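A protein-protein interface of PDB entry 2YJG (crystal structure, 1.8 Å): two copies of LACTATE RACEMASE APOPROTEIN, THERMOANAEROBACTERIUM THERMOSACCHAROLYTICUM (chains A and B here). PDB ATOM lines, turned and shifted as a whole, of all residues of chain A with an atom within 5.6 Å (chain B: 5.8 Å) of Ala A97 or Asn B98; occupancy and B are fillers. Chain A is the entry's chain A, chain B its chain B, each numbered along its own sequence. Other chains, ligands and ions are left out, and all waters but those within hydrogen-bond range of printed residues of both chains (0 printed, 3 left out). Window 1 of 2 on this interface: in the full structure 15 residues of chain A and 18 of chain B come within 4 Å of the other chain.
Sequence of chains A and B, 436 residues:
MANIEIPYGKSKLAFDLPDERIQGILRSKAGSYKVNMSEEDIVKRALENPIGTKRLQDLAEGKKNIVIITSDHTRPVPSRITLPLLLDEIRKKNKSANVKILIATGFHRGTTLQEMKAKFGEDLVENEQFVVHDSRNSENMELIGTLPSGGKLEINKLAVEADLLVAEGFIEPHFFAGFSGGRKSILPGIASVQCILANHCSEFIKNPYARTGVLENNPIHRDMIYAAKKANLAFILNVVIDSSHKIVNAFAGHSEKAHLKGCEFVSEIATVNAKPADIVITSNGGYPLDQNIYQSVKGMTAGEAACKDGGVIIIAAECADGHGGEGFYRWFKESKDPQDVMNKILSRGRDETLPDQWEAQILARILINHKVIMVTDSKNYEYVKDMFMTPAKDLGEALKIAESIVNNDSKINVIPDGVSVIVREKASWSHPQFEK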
ATOM      1  N   ALA A  60      12.096 -11.590  25.709  1.00  0.00           N
ATOM      2  CA  ALA A  60      13.006 -11.857  24.601  1.00  0.00           C
ATOM      3  C   ALA A  60      14.409 -12.299  25.078  1.00  0.00           C
ATOM      4  O   ALA A  60      15.244 -12.739  24.283  1.00  0.00           O
ATOM      5  CB  ALA A  60      13.170 -10.573  23.788  1.00  0.00           C
ATOM      6  N   LYS A  63      16.287 -15.753  24.065  1.00  0.00           N
ATOM      7  CA  LYS A  63      15.574 -16.429  22.979  1.00  0.00           C
ATOM      8  C   LYS A  63      16.403 -16.358  21.710  1.00  0.00           C
ATOM      9  O   LYS A  63      17.049 -15.329  21.471  1.00  0.00           O
ATOM     10  CB  LYS A  63      14.240 -15.736  22.706  1.00  0.00           C
ATOM     11  CG  LYS A  63      13.287 -15.719  23.908  1.00  0.00           C
ATOM     12  CD  LYS A  63      12.792 -17.075  24.253  1.00  0.00           C
ATOM     13  CE  LYS A  63      11.479 -17.057  24.997  1.00  0.00           C
ATOM     14  NZ  LYS A  63      11.689 -17.106  26.455  1.00  0.00           N
ATOM     15  N   ILE A  66      13.196 -15.190  17.258  1.00  0.00           N
ATOM     16  CA  ILE A  66      12.022 -14.333  17.468  1.00  0.00           C
ATOM     17  C   ILE A  66      11.334 -13.952  16.161  1.00  0.00           C
ATOM     18  O   ILE A  66      11.986 -13.707  15.158  1.00  0.00           O
ATOM     19  CB  ILE A  66      12.427 -13.080  18.235  1.00  0.00           C
ATOM     20  CG1 ILE A  66      13.162 -13.506  19.507  1.00  0.00           C
ATOM     21  CG2 ILE A  66      11.217 -12.210  18.570  1.00  0.00           C
ATOM     22  CD1 ILE A  66      13.711 -12.385  20.312  1.00  0.00           C
ATOM     23  N   ILE A  90      13.198  -5.602  22.096  1.00  0.00           N
ATOM     24  CA  ILE A  90      13.707  -6.954  21.951  1.00  0.00           C
ATOM     25  C   ILE A  90      15.229  -7.070  22.214  1.00  0.00           C
ATOM     26  O   ILE A  90      15.643  -8.064  22.797  1.00  0.00           O
ATOM     27  CB  ILE A  90      13.373  -7.517  20.559  1.00  0.00           C
ATOM     28  CG1 ILE A  90      11.863  -7.866  20.481  1.00  0.00           C
ATOM     29  CG2 ILE A  90      14.203  -8.764  20.237  1.00  0.00           C
ATOM     30  CD1 ILE A  90      11.234  -7.992  19.045  1.00  0.00           C
ATOM     31  N   ARG A  91      16.003  -6.098  21.769  1.00  0.00           N
ATOM     32  CA  ARG A  91      17.480  -6.192  21.785  1.00  0.00           C
ATOM     33  C   ARG A  91      18.068  -5.709  23.101  1.00  0.00           C
ATOM     34  O   ARG A  91      19.257  -5.955  23.383  1.00  0.00           O
ATOM     35  CB  ARG A  91      18.083  -5.450  20.596  1.00  0.00           C
ATOM     36  CG  ARG A  91      17.823  -6.228  19.283  1.00  0.00           C
ATOM     37  CD  ARG A  91      18.268  -5.456  18.004  1.00  0.00           C
ATOM     38  NE  ARG A  91      18.204  -6.336  16.850  1.00  0.00           N
ATOM     39  CZ  ARG A  91      17.783  -6.031  15.633  1.00  0.00           C
ATOM     40  NH1 ARG A  91      17.305  -4.827  15.319  1.00  0.00           N
ATOM     41  NH2 ARG A  91      17.806  -6.976  14.704  1.00  0.00           N
ATOM     42  N   ASN A  94      19.134  -8.696  24.758  1.00  0.00           N
ATOM     43  CA  ASN A  94      19.432  -9.743  23.784  1.00  0.00           C
ATOM     44  C   ASN A  94      19.969  -9.106  22.471  1.00  0.00           C
ATOM     45  O   ASN A  94      19.282  -9.075  21.410  1.00  0.00           O
ATOM     46  CB  ASN A  94      18.169 -10.586  23.563  1.00  0.00           C
ATOM     47  CG  ASN A  94      18.422 -11.843  22.818  1.00  0.00           C
ATOM     48  OD1 ASN A  94      19.531 -12.084  22.345  1.00  0.00           O
ATOM     49  ND2 ASN A  94      17.390 -12.672  22.687  1.00  0.00           N
ATOM     50  N   LYS A  95      21.204  -8.587  22.522  1.00  0.00           N
ATOM     51  CA  LYS A  95      21.647  -7.723  21.457  1.00  0.00           C
ATOM     52  C   LYS A  95      21.740  -8.487  20.144  1.00  0.00           C
ATOM     53  O   LYS A  95      21.529  -7.892  19.102  1.00  0.00           O
ATOM     54  CB  LYS A  95      22.996  -7.038  21.732  1.00  0.00           C
ATOM     55  CG  LYS A  95      22.935  -5.980  22.845  1.00  0.00           C
ATOM     56  CD  LYS A  95      22.170  -4.739  22.475  1.00  0.00           C
ATOM     57  CE  LYS A  95      21.880  -3.895  23.727  1.00  0.00           C
ATOM     58  NZ  LYS A  95      21.627  -2.515  23.284  1.00  0.00           N
ATOM     59  N   SER A  96      22.020  -9.790  20.224  1.00  0.00           N
ATOM     60  CA  SER A  96      22.248 -10.638  19.051  1.00  0.00           C
ATOM     61  C   SER A  96      21.040 -11.492  18.676  1.00  0.00           C
ATOM     62  O   SER A  96      21.165 -12.446  17.927  1.00  0.00           O
ATOM     63  CB  SER A  96      23.460 -11.567  19.333  1.00  0.00           C
ATOM     64  OG  SER A  96      24.594 -10.768  19.637  1.00  0.00           O
ATOM     65  N   ALA A  97      19.858 -11.136  19.179  1.00  0.00           N
ATOM     66  CA  ALA A  97      18.635 -11.837  18.810  1.00  0.00           C
ATOM     67  C   ALA A  97      18.432 -11.916  17.321  1.00  0.00           C
ATOM     68  O   ALA A  97      18.643 -10.951  16.583  1.00  0.00           O
ATOM     69  CB  ALA A  97      17.390 -11.174  19.449  1.00  0.00           C
ATOM     70  N   ASN A  98      18.054 -13.104  16.888  1.00  0.00           N
ATOM     71  CA  ASN A  98      17.522 -13.259  15.572  1.00  0.00           C
ATOM     72  C   ASN A  98      16.073 -12.851  15.604  1.00  0.00           C
ATOM     73  O   ASN A  98      15.266 -13.415  16.380  1.00  0.00           O
ATOM     74  CB  ASN A  98      17.624 -14.680  15.103  1.00  0.00           C
ATOM     75  CG  ASN A  98      19.017 -15.133  15.004  1.00  0.00           C
ATOM     76  OD1 ASN A  98      19.418 -16.069  15.706  1.00  0.00           O
ATOM     77  ND2 ASN A  98      19.808 -14.429  14.196  1.00  0.00           N
ATOM     78  N   VAL A  99      15.729 -11.934  14.722  1.00  0.00           N
ATOM     79  CA  VAL A  99      14.365 -11.413  14.674  1.00  0.00           C
ATOM     80  C   VAL A  99      13.886 -11.410  13.238  1.00  0.00           C
ATOM     81  O   VAL A  99      14.450 -10.706  12.413  1.00  0.00           O
ATOM     82  CB  VAL A  99      14.236 -10.017  15.236  1.00  0.00           C
ATOM     83  CG1 VAL A  99      12.704  -9.563  15.285  1.00  0.00           C
ATOM     84  CG2 VAL A  99      14.773  -9.945  16.572  1.00  0.00           C
ATOM     85  N   LYS B  63      30.010 -19.490  16.413  1.00  0.00           N
ATOM     86  CA  LYS B  63      30.124 -18.022  16.255  1.00  0.00           C
ATOM     87  C   LYS B  63      28.725 -17.438  16.085  1.00  0.00           C
ATOM     88  O   LYS B  63      27.999 -17.818  15.143  1.00  0.00           O
ATOM     89  CB  LYS B  63      30.991 -17.650  15.025  1.00  0.00           C
ATOM     90  CG  LYS B  63      32.288 -18.384  14.880  1.00  0.00           C
ATOM     91  CD  LYS B  63      33.419 -17.844  15.726  1.00  0.00           C
ATOM     92  CE  LYS B  63      34.761 -18.388  15.233  1.00  0.00           C
ATOM     93  NZ  LYS B  63      34.901 -19.864  15.324  1.00  0.00           N
ATOM     94  N   LYS B  64      28.319 -16.563  17.025  1.00  0.00           N
ATOM     95  CA  LYS B  64      26.978 -15.998  17.032  1.00  0.00           C
ATOM     96  C   LYS B  64      26.856 -14.880  15.989  1.00  0.00           C
ATOM     97  O   LYS B  64      25.955 -14.920  15.204  1.00  0.00           O
ATOM     98  CB  LYS B  64      26.619 -15.479  18.446  1.00  0.00           C
ATOM     99  CG  LYS B  64      25.162 -14.979  18.618  1.00  0.00           C
ATOM    100  CD  LYS B  64      24.150 -15.841  17.792  1.00  0.00           C
ATOM    101  CE  LYS B  64      22.712 -15.689  18.260  1.00  0.00           C
ATOM    102  NZ  LYS B  64      22.013 -17.012  18.181  1.00  0.00           N
ATOM    103  N   ASN B  65      27.755 -13.881  15.985  1.00  0.00           N
ATOM    104  CA  ASN B  65      27.635 -12.771  15.005  1.00  0.00           C
ATOM    105  C   ASN B  65      28.605 -12.856  13.835  1.00  0.00           C
ATOM    106  O   ASN B  65      29.815 -12.747  14.018  1.00  0.00           O
ATOM    107  CB  ASN B  65      27.786 -11.439  15.714  1.00  0.00           C
ATOM    108  CG  ASN B  65      26.651 -11.202  16.666  1.00  0.00           C
ATOM    109  OD1 ASN B  65      25.499 -11.094  16.235  1.00  0.00           O
ATOM    110  ND2 ASN B  65      26.936 -11.254  17.956  1.00  0.00           N
ATOM    111  N   ILE B  66      28.026 -13.066  12.650  1.00  0.00           N
ATOM    112  CA  ILE B  66      28.790 -13.300  11.458  1.00  0.00           C
ATOM    113  C   ILE B  66      28.450 -12.225  10.420  1.00  0.00           C
ATOM    114  O   ILE B  66      27.297 -11.852  10.267  1.00  0.00           O
ATOM    115  CB  ILE B  66      28.553 -14.720  10.904  1.00  0.00           C
ATOM    116  CG1 ILE B  66      28.989 -15.773  11.975  1.00  0.00           C
ATOM    117  CG2 ILE B  66      29.367 -14.909   9.638  1.00  0.00           C
ATOM    118  CD1 ILE B  66      28.689 -17.135  11.563  1.00  0.00           C
ATOM    119  N   VAL B  67      29.492 -11.722   9.768  1.00  0.00           N
ATOM    120  CA  VAL B  67      29.395 -10.740   8.728  1.00  0.00           C
ATOM    121  C   VAL B  67      30.028 -11.287   7.452  1.00  0.00           C
ATOM    122  O   VAL B  67      31.207 -11.686   7.452  1.00  0.00           O
ATOM    123  CB  VAL B  67      30.111  -9.429   9.118  1.00  0.00           C
ATOM    124  CG1 VAL B  67      30.103  -8.429   7.961  1.00  0.00           C
ATOM    125  CG2 VAL B  67      29.443  -8.810  10.375  1.00  0.00           C
ATOM    126  N   SER B  96      21.373 -21.020  13.872  1.00  0.00           N
ATOM    127  CA  SER B  96      20.941 -19.761  14.504  1.00  0.00           C
ATOM    128  C   SER B  96      21.984 -18.647  14.467  1.00  0.00           C
ATOM    129  O   SER B  96      21.924 -17.682  15.257  1.00  0.00           O
ATOM    130  CB  SER B  96      20.583 -20.011  15.964  1.00  0.00           C
ATOM    131  OG  SER B  96      19.365 -20.734  15.991  1.00  0.00           O
ATOM    132  N   ALA B  97      22.940 -18.800  13.568  1.00  0.00           N
ATOM    133  CA  ALA B  97      23.921 -17.785  13.330  1.00  0.00           C
ATOM    134  C   ALA B  97      23.149 -16.538  12.933  1.00  0.00           C
ATOM    135  O   ALA B  97      22.144 -16.606  12.191  1.00  0.00           O
ATOM    136  CB  ALA B  97      24.879 -18.214  12.184  1.00  0.00           C
ATOM    137  N   ASN B  98      23.601 -15.413  13.460  1.00  0.00           N
ATOM    138  CA  ASN B  98      23.077 -14.109  13.089  1.00  0.00           C
ATOM    139  C   ASN B  98      24.028 -13.517  12.035  1.00  0.00           C
ATOM    140  O   ASN B  98      25.115 -13.037  12.366  1.00  0.00           O
ATOM    141  CB  ASN B  98      23.007 -13.243  14.345  1.00  0.00           C
ATOM    142  CG  ASN B  98      22.233 -11.997  14.119  1.00  0.00           C
ATOM    143  OD1 ASN B  98      22.310 -11.416  13.049  1.00  0.00           O
ATOM    144  ND2 ASN B  98      21.487 -11.573  15.114  1.00  0.00           N
ATOM    145  N   VAL B  99      23.608 -13.554  10.782  1.00  0.00           N
ATOM    146  CA  VAL B  99      24.475 -13.202   9.640  1.00  0.00           C
ATOM    147  C   VAL B  99      24.003 -11.887   9.010  1.00  0.00           C
ATOM    148  O   VAL B  99      22.835 -11.740   8.643  1.00  0.00           O
ATOM    149  CB  VAL B  99      24.496 -14.321   8.554  1.00  0.00           C
ATOM    150  CG1 VAL B  99      25.632 -14.135   7.601  1.00  0.00           C
ATOM    151  CG2 VAL B  99      24.595 -15.726   9.206  1.00  0.00           C
ATOM    152  N   LYS B 100      24.922 -10.943   8.948  1.00  0.00           N
ATOM    153  CA  LYS B 100      24.707  -9.690   8.275  1.00  0.00           C
ATOM    154  C   LYS B 100      25.566  -9.705   7.016  1.00  0.00           C
ATOM    155  O   LYS B 100      26.653 -10.265   7.027  1.00  0.00           O
ATOM    156  CB  LYS B 100      25.017  -8.556   9.262  1.00  0.00           C
ATOM    157  CG  LYS B 100      24.016  -8.588  10.422  1.00  0.00           C
ATOM    158  CD  LYS B 100      24.163  -7.442  11.318  1.00  0.00           C
ATOM    159  CE  LYS B 100      23.225  -7.591  12.530  1.00  0.00           C
ATOM    160  NZ  LYS B 100      22.246  -6.502  12.340  1.00  0.00           N
ATOM    161  N   GLN B 129      19.654  -9.929   6.298  1.00  0.00           N
ATOM    162  CA  GLN B 129      20.034  -8.671   6.827  1.00  0.00           C
ATOM    163  C   GLN B 129      21.169  -8.108   5.957  1.00  0.00           C
ATOM    164  O   GLN B 129      22.298  -8.609   6.015  1.00  0.00           O
ATOM    165  CB  GLN B 129      20.579  -8.830   8.277  1.00  0.00           C
ATOM    166  CG  GLN B 129      19.581  -9.402   9.275  1.00  0.00           C
ATOM    167  CD  GLN B 129      20.219  -9.805  10.544  1.00  0.00           C
ATOM    168  OE1 GLN B 129      20.540 -11.022  10.751  1.00  0.00           O
ATOM    169  NE2 GLN B 129      20.491  -8.830  11.391  1.00  0.00           N
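Among the printed residues, pairs that only touch across the chains: Ser A96 with Lys B64, Asn A98 with Lys B64 and Asn A98 with Ala B97.
Ala A97 touches just one residue of chain B: Asn B98 (3.3 Å).
Of chain A, only Ser A96 (3.0 Å), Ala A97 (3.3 Å) and Asn A98 (3.4 Å) come within 4 Å of Asn B98.
Of the printed residues of chain A, Ser B96 touches Asn A98 (3.0 Å).
Printed residues of chain B within 4 Å of Asn A98: Lys B64, Ser B96, Ala B97 and Asn B98.
Ile A66 touches none of the printed residues of chain B.
The nearest residue of chain B that does not touch Ala A97 is Lys B64 (5.5 Å).
Along chain A the printed residues that touch a printed residue of chain B span positions 96 to 98.
Ser A96 touches Asn B98, and with the chains exchanged Asn A98 touches Ser B96.
Ala A97 touches Asn B98, and with the chains exchanged Asn A98 touches Ala B97.
Asn A98 touches its own counterpart, Asn B98.
Positions printed for both chains: 63, 66, 96, 97, 98 and 99.
Of the 8 pairs that touch across the chains among the printed residues, 5 have their exchanged pair printed and touching as well.
The side-chain hydroxyl (OG) of Ser A96 lies within hydrogen-bond range of the side-chain amide nitrogen (ND2) of Asn B65, at 2.9 Å.
The backbone carbonyl oxygen of Ser A96 lies within hydrogen-bond range of the side-chain amide nitrogen of Asn B98 (3.0 Å).
The side-chain amide nitrogen (ND2) of Asn B98 sits at hydrogen-bond distance from the backbone carbonyl oxygen (O) of Ala A97 (3.3 Å).
O of Ser B96 lies close to OD1 of Asn A98 (3.0 Å).
ND2 of Asn B98 sits close to ND2 of Asn A98, 3.4 Å away.
N of Ile A66 sits at hydrogen-bond distance from O of Asn A98 (2.9 Å).
The backbone NH (N) of Ala A97 sits at hydrogen-bond distance from the side-chain amide oxygen (OD1) of Asn A94.
O of Ser B96 lies within hydrogen-bond range of NZ of Lys B64 (3.0 Å).
The backbone NH of Asn B98 lies within hydrogen-bond range of the backbone carbonyl oxygen of Lys B64, at 3.0 Å.
The backbone NH of Ile B66 is in hydrogen-bond range of the backbone carbonyl oxygen of Asn B98.
The side-chain amide oxygen (OD1) of Asn B98 lies close to the side-chain amide oxygen (OE1) of Gln B129 (2.9 Å).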
